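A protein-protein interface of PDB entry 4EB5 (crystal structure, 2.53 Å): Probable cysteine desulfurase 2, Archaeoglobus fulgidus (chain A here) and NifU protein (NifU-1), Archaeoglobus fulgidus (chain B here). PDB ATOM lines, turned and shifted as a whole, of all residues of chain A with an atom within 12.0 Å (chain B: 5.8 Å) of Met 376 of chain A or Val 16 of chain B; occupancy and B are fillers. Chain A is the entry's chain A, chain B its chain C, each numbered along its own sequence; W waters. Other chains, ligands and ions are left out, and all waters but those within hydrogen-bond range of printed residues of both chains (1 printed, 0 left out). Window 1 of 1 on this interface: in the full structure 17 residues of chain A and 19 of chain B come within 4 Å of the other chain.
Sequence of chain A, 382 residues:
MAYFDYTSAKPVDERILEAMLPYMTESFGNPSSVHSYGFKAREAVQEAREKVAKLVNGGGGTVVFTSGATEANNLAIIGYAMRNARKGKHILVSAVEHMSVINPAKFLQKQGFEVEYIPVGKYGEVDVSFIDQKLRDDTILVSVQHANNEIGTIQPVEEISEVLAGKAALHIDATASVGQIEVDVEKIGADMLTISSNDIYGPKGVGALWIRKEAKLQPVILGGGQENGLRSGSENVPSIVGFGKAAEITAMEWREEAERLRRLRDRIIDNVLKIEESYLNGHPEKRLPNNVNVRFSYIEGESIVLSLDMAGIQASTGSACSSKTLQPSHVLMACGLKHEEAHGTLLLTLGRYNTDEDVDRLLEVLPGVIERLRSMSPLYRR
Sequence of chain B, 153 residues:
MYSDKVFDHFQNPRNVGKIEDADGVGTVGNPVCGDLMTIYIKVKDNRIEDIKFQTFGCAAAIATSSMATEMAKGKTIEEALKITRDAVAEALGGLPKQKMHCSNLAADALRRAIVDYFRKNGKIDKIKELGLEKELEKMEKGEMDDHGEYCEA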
ATOM      1  N   SER A 297       3.989  13.364  33.426  1.00  0.00           N
ATOM      2  CA  SER A 297       5.007  14.358  33.088  1.00  0.00           C
ATOM      3  C   SER A 297       4.478  15.307  32.025  1.00  0.00           C
ATOM      4  O   SER A 297       3.542  14.971  31.283  1.00  0.00           O
ATOM      5  CB  SER A 297       6.264  13.687  32.548  1.00  0.00           C
ATOM      6  OG  SER A 297       6.774  12.690  33.408  1.00  0.00           O
ATOM      7  N   TYR A 298       5.109  16.484  31.965  1.00  0.00           N
ATOM      8  CA  TYR A 298       4.921  17.507  30.924  1.00  0.00           C
ATOM      9  C   TYR A 298       3.646  18.330  30.983  1.00  0.00           C
ATOM     10  O   TYR A 298       3.506  19.321  30.228  1.00  0.00           O
ATOM     11  CB  TYR A 298       5.070  16.939  29.503  1.00  0.00           C
ATOM     12  CG  TYR A 298       6.110  15.877  29.338  1.00  0.00           C
ATOM     13  CD1 TYR A 298       7.450  16.127  29.619  1.00  0.00           C
ATOM     14  CD2 TYR A 298       5.744  14.602  28.895  1.00  0.00           C
ATOM     15  CE1 TYR A 298       8.421  15.119  29.457  1.00  0.00           C
ATOM     16  CE2 TYR A 298       6.691  13.595  28.733  1.00  0.00           C
ATOM     17  CZ  TYR A 298       8.024  13.860  29.002  1.00  0.00           C
ATOM     18  OH  TYR A 298       8.947  12.853  28.835  1.00  0.00           O
ATOM     19  N   ILE A 299       2.715  17.954  31.853  1.00  0.00           N
ATOM     20  CA  ILE A 299       1.509  18.777  31.989  1.00  0.00           C
ATOM     21  C   ILE A 299       1.182  19.215  33.427  1.00  0.00           C
ATOM     22  O   ILE A 299       1.742  18.710  34.399  1.00  0.00           O
ATOM     23  CB  ILE A 299       0.320  18.117  31.317  1.00  0.00           C
ATOM     24  CG1 ILE A 299       0.090  16.726  31.921  1.00  0.00           C
ATOM     25  CG2 ILE A 299       0.570  18.077  29.791  1.00  0.00           C
ATOM     26  CD1 ILE A 299      -1.167  16.025  31.465  1.00  0.00           C
ATOM     27  N   GLU A 300       0.249  20.158  33.534  1.00  0.00           N
ATOM     28  CA  GLU A 300      -0.117  20.754  34.794  1.00  0.00           C
ATOM     29  C   GLU A 300      -1.468  20.222  35.346  1.00  0.00           C
ATOM     30  O   GLU A 300      -2.473  20.111  34.612  1.00  0.00           O
ATOM     31  CB  GLU A 300      -0.136  22.265  34.612  1.00  0.00           C
ATOM     32  CG  GLU A 300      -0.218  23.060  35.892  1.00  0.00           C
ATOM     33  CD  GLU A 300      -1.602  23.101  36.447  1.00  0.00           C
ATOM     34  OE1 GLU A 300      -1.777  22.893  37.680  1.00  0.00           O
ATOM     35  OE2 GLU A 300      -2.528  23.311  35.631  1.00  0.00           O
ATOM     36  N   GLY A 301      -1.467  19.955  36.664  1.00  0.00           N
ATOM     37  CA  GLY A 301      -2.598  19.404  37.437  1.00  0.00           C
ATOM     38  C   GLY A 301      -3.969  20.040  37.402  1.00  0.00           C
ATOM     39  O   GLY A 301      -4.964  19.355  37.166  1.00  0.00           O
ATOM     40  N   GLU A 302      -4.055  21.333  37.659  1.00  0.00           N
ATOM     41  CA  GLU A 302      -5.342  22.027  37.506  1.00  0.00           C
ATOM     42  C   GLU A 302      -5.978  21.810  36.087  1.00  0.00           C
ATOM     43  O   GLU A 302      -7.183  21.641  35.978  1.00  0.00           O
ATOM     44  CB  GLU A 302      -5.233  23.526  37.881  1.00  0.00           C
ATOM     45  CG  GLU A 302      -6.578  24.272  37.783  1.00  0.00           C
ATOM     46  CD  GLU A 302      -6.457  25.790  37.678  1.00  0.00           C
ATOM     47  OE1 GLU A 302      -6.596  26.375  36.560  1.00  0.00           O
ATOM     48  OE2 GLU A 302      -6.243  26.412  38.722  1.00  0.00           O
ATOM     49  N   SER A 303      -5.160  21.789  35.036  1.00  0.00           N
ATOM     50  CA  SER A 303      -5.629  21.578  33.656  1.00  0.00           C
ATOM     51  C   SER A 303      -6.127  20.166  33.371  1.00  0.00           C
ATOM     52  O   SER A 303      -7.081  20.012  32.614  1.00  0.00           O
ATOM     53  CB  SER A 303      -4.537  21.928  32.645  1.00  0.00           C
ATOM     54  OG  SER A 303      -4.360  23.324  32.536  1.00  0.00           O
ATOM     55  N   ILE A 304      -5.495  19.146  33.956  1.00  0.00           N
ATOM     56  CA  ILE A 304      -6.044  17.786  33.900  1.00  0.00           C
ATOM     57  C   ILE A 304      -7.400  17.758  34.598  1.00  0.00           C
ATOM     58  O   ILE A 304      -8.360  17.225  34.071  1.00  0.00           O
ATOM     59  CB  ILE A 304      -5.140  16.745  34.566  1.00  0.00           C
ATOM     60  CG1 ILE A 304      -3.778  16.676  33.901  1.00  0.00           C
ATOM     61  CG2 ILE A 304      -5.771  15.364  34.494  1.00  0.00           C
ATOM     62  CD1 ILE A 304      -2.658  16.333  34.896  1.00  0.00           C
ATOM     63  N   LEU A 306      -9.635  20.054  35.234  1.00  0.00           N
ATOM     64  CA  LEU A 306     -10.720  20.808  34.581  1.00  0.00           C
ATOM     65  C   LEU A 306     -11.129  20.249  33.231  1.00  0.00           C
ATOM     66  O   LEU A 306     -12.248  20.500  32.779  1.00  0.00           O
ATOM     67  CB  LEU A 306     -10.396  22.305  34.470  1.00  0.00           C
ATOM     68  CG  LEU A 306     -10.853  23.097  35.679  1.00  0.00           C
ATOM     69  CD1 LEU A 306      -9.971  24.322  35.912  1.00  0.00           C
ATOM     70  CD2 LEU A 306     -12.289  23.492  35.405  1.00  0.00           C
ATOM     71  N   SER A 307     -10.219  19.519  32.580  1.00  0.00           N
ATOM     72  CA  SER A 307     -10.542  18.847  31.320  1.00  0.00           C
ATOM     73  C   SER A 307     -11.510  17.715  31.654  1.00  0.00           C
ATOM     74  O   SER A 307     -12.556  17.556  31.008  1.00  0.00           O
ATOM     75  CB  SER A 307      -9.286  18.265  30.643  1.00  0.00           C
ATOM     76  OG  SER A 307      -8.342  19.258  30.236  1.00  0.00           O
ATOM     77  N   MET A 310     -15.020  19.122  32.335  1.00  0.00           N
ATOM     78  CA  MET A 310     -15.816  19.318  31.089  1.00  0.00           C
ATOM     79  C   MET A 310     -16.394  18.036  30.501  1.00  0.00           C
ATOM     80  O   MET A 310     -17.451  18.080  29.925  1.00  0.00           O
ATOM     81  CB  MET A 310     -15.068  20.112  30.021  1.00  0.00           C
ATOM     82  CG  MET A 310     -15.532  21.588  29.974  1.00  0.00           C
ATOM     83  SD  MET A 310     -14.229  22.870  29.777  1.00  0.00           S
ATOM     84  CE  MET A 310     -15.279  24.331  29.572  1.00  0.00           C
ATOM     85  N   PRO A 367      -6.937   9.105  28.656  1.00  0.00           N
ATOM     86  CA  PRO A 367      -5.812   9.131  27.684  1.00  0.00           C
ATOM     87  C   PRO A 367      -5.859  10.305  26.704  1.00  0.00           C
ATOM     88  O   PRO A 367      -4.830  10.839  26.365  1.00  0.00           O
ATOM     89  CB  PRO A 367      -5.957   7.807  26.936  1.00  0.00           C
ATOM     90  CG  PRO A 367      -6.704   6.894  27.889  1.00  0.00           C
ATOM     91  CD  PRO A 367      -7.410   7.728  28.921  1.00  0.00           C
ATOM     92  N   GLY A 368      -7.047  10.736  26.316  1.00  0.00           N
ATOM     93  CA  GLY A 368      -7.189  11.825  25.369  1.00  0.00           C
ATOM     94  C   GLY A 368      -6.910  13.187  25.955  1.00  0.00           C
ATOM     95  O   GLY A 368      -6.393  14.073  25.265  1.00  0.00           O
ATOM     96  N   VAL A 369      -7.295  13.366  27.216  1.00  0.00           N
ATOM     97  CA  VAL A 369      -6.955  14.561  27.977  1.00  0.00           C
ATOM     98  C   VAL A 369      -5.437  14.706  28.091  1.00  0.00           C
ATOM     99  O   VAL A 369      -4.880  15.788  27.876  1.00  0.00           O
ATOM    100  CB  VAL A 369      -7.559  14.482  29.394  1.00  0.00           C
ATOM    101  CG1 VAL A 369      -6.929  15.549  30.361  1.00  0.00           C
ATOM    102  CG2 VAL A 369      -9.067  14.614  29.307  1.00  0.00           C
ATOM    103  N   ILE A 370      -4.777  13.616  28.460  1.00  0.00           N
ATOM    104  CA  ILE A 370      -3.346  13.656  28.636  1.00  0.00           C
ATOM    105  C   ILE A 370      -2.762  14.062  27.278  1.00  0.00           C
ATOM    106  O   ILE A 370      -2.015  15.063  27.200  1.00  0.00           O
ATOM    107  CB  ILE A 370      -2.756  12.283  29.114  1.00  0.00           C
ATOM    108  CG1 ILE A 370      -3.395  11.796  30.435  1.00  0.00           C
ATOM    109  CG2 ILE A 370      -1.243  12.339  29.176  1.00  0.00           C
ATOM    110  CD1 ILE A 370      -3.382  12.769  31.608  1.00  0.00           C
ATOM    111  N   GLU A 371      -3.124  13.313  26.217  1.00  0.00           N
ATOM    112  CA  GLU A 371      -2.588  13.598  24.866  1.00  0.00           C
ATOM    113  C   GLU A 371      -2.879  15.044  24.397  1.00  0.00           C
ATOM    114  O   GLU A 371      -2.018  15.722  23.855  1.00  0.00           O
ATOM    115  CB  GLU A 371      -3.057  12.563  23.845  1.00  0.00           C
ATOM    116  N   ARG A 372      -4.076  15.536  24.661  1.00  0.00           N
ATOM    117  CA  ARG A 372      -4.397  16.898  24.265  1.00  0.00           C
ATOM    118  C   ARG A 372      -3.498  17.932  24.914  1.00  0.00           C
ATOM    119  O   ARG A 372      -2.864  18.723  24.212  1.00  0.00           O
ATOM    120  CB  ARG A 372      -5.873  17.222  24.451  1.00  0.00           C
ATOM    121  CG  ARG A 372      -6.682  16.917  23.182  1.00  0.00           C
ATOM    122  CD  ARG A 372      -8.175  17.254  23.387  1.00  0.00           C
ATOM    123  NE  ARG A 372      -8.875  16.185  24.108  1.00  0.00           N
ATOM    124  N   LEU A 373      -3.400  17.872  26.239  1.00  0.00           N
ATOM    125  CA  LEU A 373      -2.552  18.765  26.997  1.00  0.00           C
ATOM    126  C   LEU A 373      -1.111  18.591  26.611  1.00  0.00           C
ATOM    127  O   LEU A 373      -0.386  19.567  26.468  1.00  0.00           O
ATOM    128  CB  LEU A 373      -2.738  18.545  28.503  1.00  0.00           C
ATOM    129  CG  LEU A 373      -4.139  18.906  29.003  1.00  0.00           C
ATOM    130  CD1 LEU A 373      -4.385  18.273  30.371  1.00  0.00           C
ATOM    131  CD2 LEU A 373      -4.279  20.404  29.060  1.00  0.00           C
ATOM    132  N   ARG A 374      -0.681  17.360  26.440  1.00  0.00           N
ATOM    133  CA  ARG A 374       0.687  17.156  26.040  1.00  0.00           C
ATOM    134  C   ARG A 374       1.050  17.812  24.710  1.00  0.00           C
ATOM    135  O   ARG A 374       2.154  18.316  24.561  1.00  0.00           O
ATOM    136  CB  ARG A 374       1.037  15.680  26.032  1.00  0.00           C
ATOM    137  CG  ARG A 374       1.942  15.293  27.186  1.00  0.00           C
ATOM    138  CD  ARG A 374       1.704  13.885  27.611  1.00  0.00           C
ATOM    139  NE  ARG A 374       2.287  13.647  28.914  1.00  0.00           N
ATOM    140  CZ  ARG A 374       2.395  12.455  29.485  1.00  0.00           C
ATOM    141  NH1 ARG A 374       2.979  12.351  30.672  1.00  0.00           N
ATOM    142  NH2 ARG A 374       1.944  11.368  28.862  1.00  0.00           N
ATOM    143  N   SER A 375       0.121  17.819  23.752  1.00  0.00           N
ATOM    144  CA  SER A 375       0.411  18.360  22.442  1.00  0.00           C
ATOM    145  C   SER A 375       0.605  19.867  22.563  1.00  0.00           C
ATOM    146  O   SER A 375       1.376  20.450  21.811  1.00  0.00           O
ATOM    147  CB  SER A 375      -0.678  18.006  21.427  1.00  0.00           C
ATOM    148  OG  SER A 375      -1.805  18.873  21.568  1.00  0.00           O
ATOM    149  N   MET A 376      -0.043  20.502  23.535  1.00  0.00           N
ATOM    150  CA  MET A 376       0.256  21.918  23.773  1.00  0.00           C
ATOM    151  C   MET A 376       1.434  22.277  24.723  1.00  0.00           C
ATOM    152  O   MET A 376       1.678  23.448  24.973  1.00  0.00           O
ATOM    153  CB  MET A 376      -1.018  22.714  24.110  1.00  0.00           C
ATOM    154  CG  MET A 376      -1.770  22.340  25.349  1.00  0.00           C
ATOM    155  SD  MET A 376      -3.333  23.294  25.450  1.00  0.00           S
ATOM    156  CE  MET A 376      -2.711  24.952  25.515  1.00  0.00           C
ATOM    157  N   SER A 377       2.176  21.292  25.221  1.00  0.00           N
ATOM    158  CA  SER A 377       3.181  21.609  26.230  1.00  0.00           C
ATOM    159  C   SER A 377       4.546  21.878  25.625  1.00  0.00           C
ATOM    160  O   SER A 377       5.045  21.058  24.868  1.00  0.00           O
ATOM    161  CB  SER A 377       3.276  20.530  27.309  1.00  0.00           C
ATOM    162  OG  SER A 377       4.183  20.877  28.336  1.00  0.00           O
ATOM    163  N   PRO A 378       5.163  23.026  25.984  1.00  0.00           N
ATOM    164  CA  PRO A 378       6.517  23.281  25.515  1.00  0.00           C
ATOM    165  C   PRO A 378       7.401  22.156  25.988  1.00  0.00           C
ATOM    166  O   PRO A 378       8.384  21.854  25.329  1.00  0.00           O
ATOM    167  CB  PRO A 378       6.914  24.572  26.229  1.00  0.00           C
ATOM    168  CG  PRO A 378       5.949  24.702  27.362  1.00  0.00           C
ATOM    169  CD  PRO A 378       4.706  24.038  26.952  1.00  0.00           C
ATOM    170  N   LEU A 379       7.025  21.514  27.103  1.00  0.00           N
ATOM    171  CA  LEU A 379       7.857  20.497  27.740  1.00  0.00           C
ATOM    172  C   LEU A 379       7.843  19.171  27.001  1.00  0.00           C
ATOM    173  O   LEU A 379       8.753  18.367  27.189  1.00  0.00           O
ATOM    174  CB  LEU A 379       7.434  20.267  29.197  1.00  0.00           C
ATOM    175  CG  LEU A 379       7.538  21.415  30.207  1.00  0.00           C
ATOM    176  CD1 LEU A 379       7.256  20.896  31.617  1.00  0.00           C
ATOM    177  CD2 LEU A 379       8.899  22.117  30.162  1.00  0.00           C
ATOM    178  N   TYR A 380       6.823  18.931  26.173  1.00  0.00           N
ATOM    179  CA  TYR A 380       6.695  17.618  25.532  1.00  0.00           C
ATOM    180  C   TYR A 380       7.309  17.559  24.136  1.00  0.00           C
ATOM    181  O   TYR A 380       6.826  18.226  23.225  1.00  0.00           O
ATOM    182  CB  TYR A 380       5.236  17.163  25.501  1.00  0.00           C
ATOM    183  CG  TYR A 380       5.011  15.825  24.817  1.00  0.00           C
ATOM    184  CD1 TYR A 380       4.248  15.741  23.640  1.00  0.00           C
ATOM    185  CD2 TYR A 380       5.527  14.635  25.355  1.00  0.00           C
ATOM    186  CE1 TYR A 380       4.005  14.499  23.012  1.00  0.00           C
ATOM    187  CE2 TYR A 380       5.307  13.400  24.736  1.00  0.00           C
ATOM    188  CZ  TYR A 380       4.543  13.344  23.561  1.00  0.00           C
ATOM    189  OH  TYR A 380       4.313  12.143  22.936  1.00  0.00           O
ATOM    190  N   PRO B  13      -8.889  25.867  22.753  1.00  0.00           N
ATOM    191  CA  PRO B  13      -7.834  26.882  22.656  1.00  0.00           C
ATOM    192  C   PRO B  13      -7.430  27.213  21.209  1.00  0.00           C
ATOM    193  O   PRO B  13      -7.219  26.304  20.400  1.00  0.00           O
ATOM    194  CB  PRO B  13      -6.667  26.214  23.356  1.00  0.00           C
ATOM    195  CG  PRO B  13      -6.881  24.737  23.025  1.00  0.00           C
ATOM    196  CD  PRO B  13      -8.358  24.542  23.102  1.00  0.00           C
ATOM    197  N   ARG B  14      -7.293  28.487  20.878  1.00  0.00           N
ATOM    198  CA  ARG B  14      -6.872  28.833  19.502  1.00  0.00           C
ATOM    199  C   ARG B  14      -5.343  28.905  19.263  1.00  0.00           C
ATOM    200  O   ARG B  14      -4.562  29.215  20.188  1.00  0.00           O
ATOM    201  CB  ARG B  14      -7.599  30.084  18.997  1.00  0.00           C
ATOM    202  CG  ARG B  14      -8.948  29.741  18.359  1.00  0.00           C
ATOM    203  CD  ARG B  14     -10.016  29.340  19.370  1.00  0.00           C
ATOM    204  NE  ARG B  14     -10.885  30.430  19.815  1.00  0.00           N
ATOM    205  CZ  ARG B  14     -11.692  30.357  20.878  1.00  0.00           C
ATOM    206  NH1 ARG B  14     -11.731  29.257  21.644  1.00  0.00           N
ATOM    207  NH2 ARG B  14     -12.466  31.390  21.194  1.00  0.00           N
ATOM    208  N   ASN B  15      -4.942  28.574  18.032  1.00  0.00           N
ATOM    209  CA  ASN B  15      -3.551  28.686  17.563  1.00  0.00           C
ATOM    210  C   ASN B  15      -2.511  27.849  18.317  1.00  0.00           C
ATOM    211  O   ASN B  15      -1.380  28.251  18.463  1.00  0.00           O
ATOM    212  CB  ASN B  15      -3.125  30.158  17.503  1.00  0.00           C
ATOM    213  CG  ASN B  15      -4.247  31.076  17.059  1.00  0.00           C
ATOM    214  OD1 ASN B  15      -4.552  32.077  17.735  1.00  0.00           O
ATOM    215  ND2 ASN B  15      -4.888  30.737  15.936  1.00  0.00           N
ATOM    216  N   VAL B  16      -2.911  26.680  18.785  1.00  0.00           N
ATOM    217  CA  VAL B  16      -2.007  25.725  19.397  1.00  0.00           C
ATOM    218  C   VAL B  16      -1.000  25.143  18.401  1.00  0.00           C
ATOM    219  O   VAL B  16      -1.392  24.611  17.345  1.00  0.00           O
ATOM    220  CB  VAL B  16      -2.793  24.550  20.033  1.00  0.00           C
ATOM    221  CG1 VAL B  16      -1.871  23.640  20.790  1.00  0.00           C
ATOM    222  CG2 VAL B  16      -3.860  25.077  20.961  1.00  0.00           C
ATOM    223  N   GLY B  17       0.289  25.258  18.739  1.00  0.00           N
ATOM    224  CA  GLY B  17       1.344  24.503  18.056  1.00  0.00           C
ATOM    225  C   GLY B  17       2.744  25.099  18.099  1.00  0.00           C
ATOM    226  O   GLY B  17       2.992  26.100  18.772  1.00  0.00           O
ATOM    227  N   LYS B  18       3.659  24.442  17.386  1.00  0.00           N
ATOM    228  CA  LYS B  18       4.970  24.978  17.059  1.00  0.00           C
ATOM    229  C   LYS B  18       4.944  25.678  15.688  1.00  0.00           C
ATOM    230  O   LYS B  18       3.921  25.696  15.006  1.00  0.00           O
ATOM    231  CB  LYS B  18       6.027  23.859  17.051  1.00  0.00           C
ATOM    232  CG  LYS B  18       6.742  23.620  18.380  1.00  0.00           C
ATOM    233  CD  LYS B  18       6.342  22.287  19.055  1.00  0.00           C
ATOM    234  CE  LYS B  18       7.353  21.919  20.194  1.00  0.00           C
ATOM    235  NZ  LYS B  18       6.895  20.832  21.149  1.00  0.00           N
ATOM    236  N   LYS B  52       1.614  30.819  16.675  1.00  0.00           N
ATOM    237  CA  LYS B  52       1.236  29.651  17.453  1.00  0.00           C
ATOM    238  C   LYS B  52       1.776  29.744  18.859  1.00  0.00           C
ATOM    239  O   LYS B  52       2.752  30.481  19.133  1.00  0.00           O
ATOM    240  CB  LYS B  52       1.719  28.368  16.785  1.00  0.00           C
ATOM    241  CG  LYS B  52       1.210  28.127  15.378  1.00  0.00           C
ATOM    242  CD  LYS B  52      -0.264  27.721  15.275  1.00  0.00           C
ATOM    243  CE  LYS B  52      -0.537  27.236  13.842  1.00  0.00           C
ATOM    244  NZ  LYS B  52      -1.970  26.977  13.584  1.00  0.00           N
ATOM    245  N   PHE B  53       1.149  29.007  19.768  1.00  0.00           N
ATOM    246  CA  PHE B  53       1.691  28.915  21.142  1.00  0.00           C
ATOM    247  C   PHE B  53       1.815  27.509  21.667  1.00  0.00           C
ATOM    248  O   PHE B  53       1.107  26.588  21.234  1.00  0.00           O
ATOM    249  CB  PHE B  53       0.878  29.750  22.130  1.00  0.00           C
ATOM    250  CG  PHE B  53      -0.379  29.081  22.589  1.00  0.00           C
ATOM    251  CD1 PHE B  53      -0.354  28.159  23.621  1.00  0.00           C
ATOM    252  CD2 PHE B  53      -1.603  29.364  21.978  1.00  0.00           C
ATOM    253  CE1 PHE B  53      -1.525  27.545  24.059  1.00  0.00           C
ATOM    254  CE2 PHE B  53      -2.759  28.740  22.415  1.00  0.00           C
ATOM    255  CZ  PHE B  53      -2.709  27.820  23.470  1.00  0.00           C
ATOM    256  N   GLN B  54       2.711  27.369  22.626  1.00  0.00           N
ATOM    257  CA  GLN B  54       2.858  26.160  23.410  1.00  0.00           C
ATOM    258  C   GLN B  54       2.988  26.582  24.870  1.00  0.00           C
ATOM    259  O   GLN B  54       3.945  27.286  25.240  1.00  0.00           O
ATOM    260  CB  GLN B  54       4.144  25.438  23.012  1.00  0.00           C
ATOM    261  CG  GLN B  54       4.147  24.903  21.634  1.00  0.00           C
ATOM    262  CD  GLN B  54       3.649  23.529  21.609  1.00  0.00           C
ATOM    263  OE1 GLN B  54       4.397  22.574  21.897  1.00  0.00           O
ATOM    264  NE2 GLN B  54       2.366  23.379  21.278  1.00  0.00           N
ATOM    265  N   THR B  55       2.044  26.154  25.699  1.00  0.00           N
ATOM    266  CA  THR B  55       2.043  26.576  27.098  1.00  0.00           C
ATOM    267  C   THR B  55       1.859  25.420  28.107  1.00  0.00           C
ATOM    268  O   THR B  55       1.121  24.447  27.874  1.00  0.00           O
ATOM    269  CB  THR B  55       1.033  27.733  27.366  1.00  0.00           C
ATOM    270  OG1 THR B  55       0.771  27.827  28.783  1.00  0.00           O
ATOM    271  CG2 THR B  55      -0.251  27.424  26.721  1.00  0.00           C
ATOM    272  N   PHE B  56       2.560  25.559  29.224  1.00  0.00           N
ATOM    273  CA  PHE B  56       2.566  24.603  30.321  1.00  0.00           C
ATOM    274  C   PHE B  56       2.047  25.339  31.539  1.00  0.00           C
ATOM    275  O   PHE B  56       2.724  26.199  32.113  1.00  0.00           O
ATOM    276  CB  PHE B  56       3.983  24.145  30.570  1.00  0.00           C
ATOM    277  CG  PHE B  56       4.169  23.407  31.857  1.00  0.00           C
ATOM    278  CD1 PHE B  56       3.774  22.076  31.978  1.00  0.00           C
ATOM    279  CD2 PHE B  56       4.792  24.032  32.952  1.00  0.00           C
ATOM    280  CE1 PHE B  56       3.984  21.372  33.165  1.00  0.00           C
ATOM    281  CE2 PHE B  56       5.001  23.342  34.128  1.00  0.00           C
ATOM    282  CZ  PHE B  56       4.589  22.004  34.231  1.00  0.00           C
ATOM    283  N   ILE B  62      -3.808  28.792  29.798  1.00  0.00           N
ATOM    284  CA  ILE B  62      -4.155  28.349  28.466  1.00  0.00           C
ATOM    285  C   ILE B  62      -5.125  29.362  27.801  1.00  0.00           C
ATOM    286  O   ILE B  62      -5.018  29.664  26.627  1.00  0.00           O
ATOM    287  CB  ILE B  62      -4.677  26.899  28.501  1.00  0.00           C
ATOM    288  CG1 ILE B  62      -3.511  25.945  28.774  1.00  0.00           C
ATOM    289  CG2 ILE B  62      -5.380  26.507  27.181  1.00  0.00           C
ATOM    290  CD1 ILE B  62      -3.963  24.534  29.000  1.00  0.00           C
HETATM  291  O   HOH W   1      -0.081  21.809  28.241  1.00  0.00           O
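The backbone carbonyl oxygen (O) of Tyr 380 of chain A is in hydrogen-bond range of the side-chain amino group (NZ) of Lys 18 of chain B (3.3 Å). The backbone carbonyl oxygen of Ser 377 of chain A sits close to the side-chain amide oxygen of Gln 54 of chain B. O of Met 376 of chain A is in hydrogen-bond range of N of Thr 55 of chain B, at 2.8 Å. The backbone carbonyl oxygen (O) of Ser 375 of chain A sits at hydrogen-bond distance from the side-chain amide nitrogen (NE2) of Gln 54 of chain B (3.1 Å).
The backbone carbonyl oxygen (O) of Tyr 298 of chain A sits at hydrogen-bond distance from the side-chain hydroxyl (OG) of Ser 377 of chain A, at 2.5 Å. The side-chain hydroxyl of Ser 375 of chain A lies within hydrogen-bond range of the backbone carbonyl oxygen of Arg 372 of chain A. The side-chain carboxylate of Glu 300 of chain A is in hydrogen-bond range of the backbone NH of Glu 302 of chain A (2.8 Å). The backbone carbonyl oxygen (O) of Ser 303 of chain A is in hydrogen-bond range of the side-chain hydroxyl (OG) of Ser 307 of chain A, 2.8 Å away. OE1 of Gln 54 of chain B lies within hydrogen-bond range of NZ of Lys 18 of chain B.
Tyr 298 of chain A touches Phe 56 of chain B (O to CD1, 3.3 Å). Ile 299 of chain A touches Phe 56 of chain B. Ser 303 of chain A touches Ile 62 of chain B. Met 376 of chain A touches Val 16 of chain B (CB to CG1, 3.6 Å). Met 376 of chain A touches Phe 53 of chain B (CE to CE1, 3.2 Å). Met 376 of chain A touches Gln 54 of chain B (O to CA, 3.3 Å). CG1 of Ile 62 of chain B touches CE of Met 376 of chain A, at 3.5 Å. Ser 377 of chain A touches Thr 55 of chain B (CA to O, 3.9 Å). CD1 of Phe 56 of chain B touches OG of Ser 377 of chain A (3.9 Å). CD of Pro 378 of chain A touches C of Gln 54 of chain B (3.7 Å).
Of the printed residues of chain B, Ile 299 of chain A touches Phe 56. Of the printed residues of chain B, Glu 300 of chain A touches Phe 56. Arg 372 of chain A touches none of the printed residues of chain B. Met 376 of chain A touches just these residues of chain B: Val 16, Phe 53, Gln 54, Thr 55 and Ile 62. No residue of chain A comes within 4 Å of Pro 13 of chain B. Val 16 of chain B touches just one residue of chain A: Met 376. No residue of chain A comes within 4 Å of Gly 17 of chain B. Lys 18 of chain B touches just one residue of chain A: Tyr 380. Of chain A, only Met 376 comes within 4 Å of Phe 53 of chain B. Of chain A, only Ser 375, Met 376, Ser 377 and Pro 378 come within 4 Å of Gln 54 of chain B. Of the printed residues of chain A, Phe 56 of chain B touches Tyr 298, Ile 299, Glu 300, Ser 377, Pro 378 and Leu 379. Ile 62 of chain B touches just these residues of chain A: Ser 303 and Met 376. The nearest residue of chain A that does not touch Val 16 of chain B is Ser 375 of chain A (4.7 Å). The nearest printed residue of chain B that does not touch Ser 375 of chain A is Val 16 of chain B (4.7 Å).
Of the 12 printed residues of chain B, 7 touch a printed residue of chain A. Hydrophobic or aromatic side chains of chain B within 4 Å of the printed part of chain A: Val 16, Phe 53, Phe 56 and Ile 62. Among the printed residues, 18 pairs touch across the chains.
Water W1 bridges O of Leu 373 of chain A (2.9 Å) and O of Thr 55 of chain B (2.9 Å).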
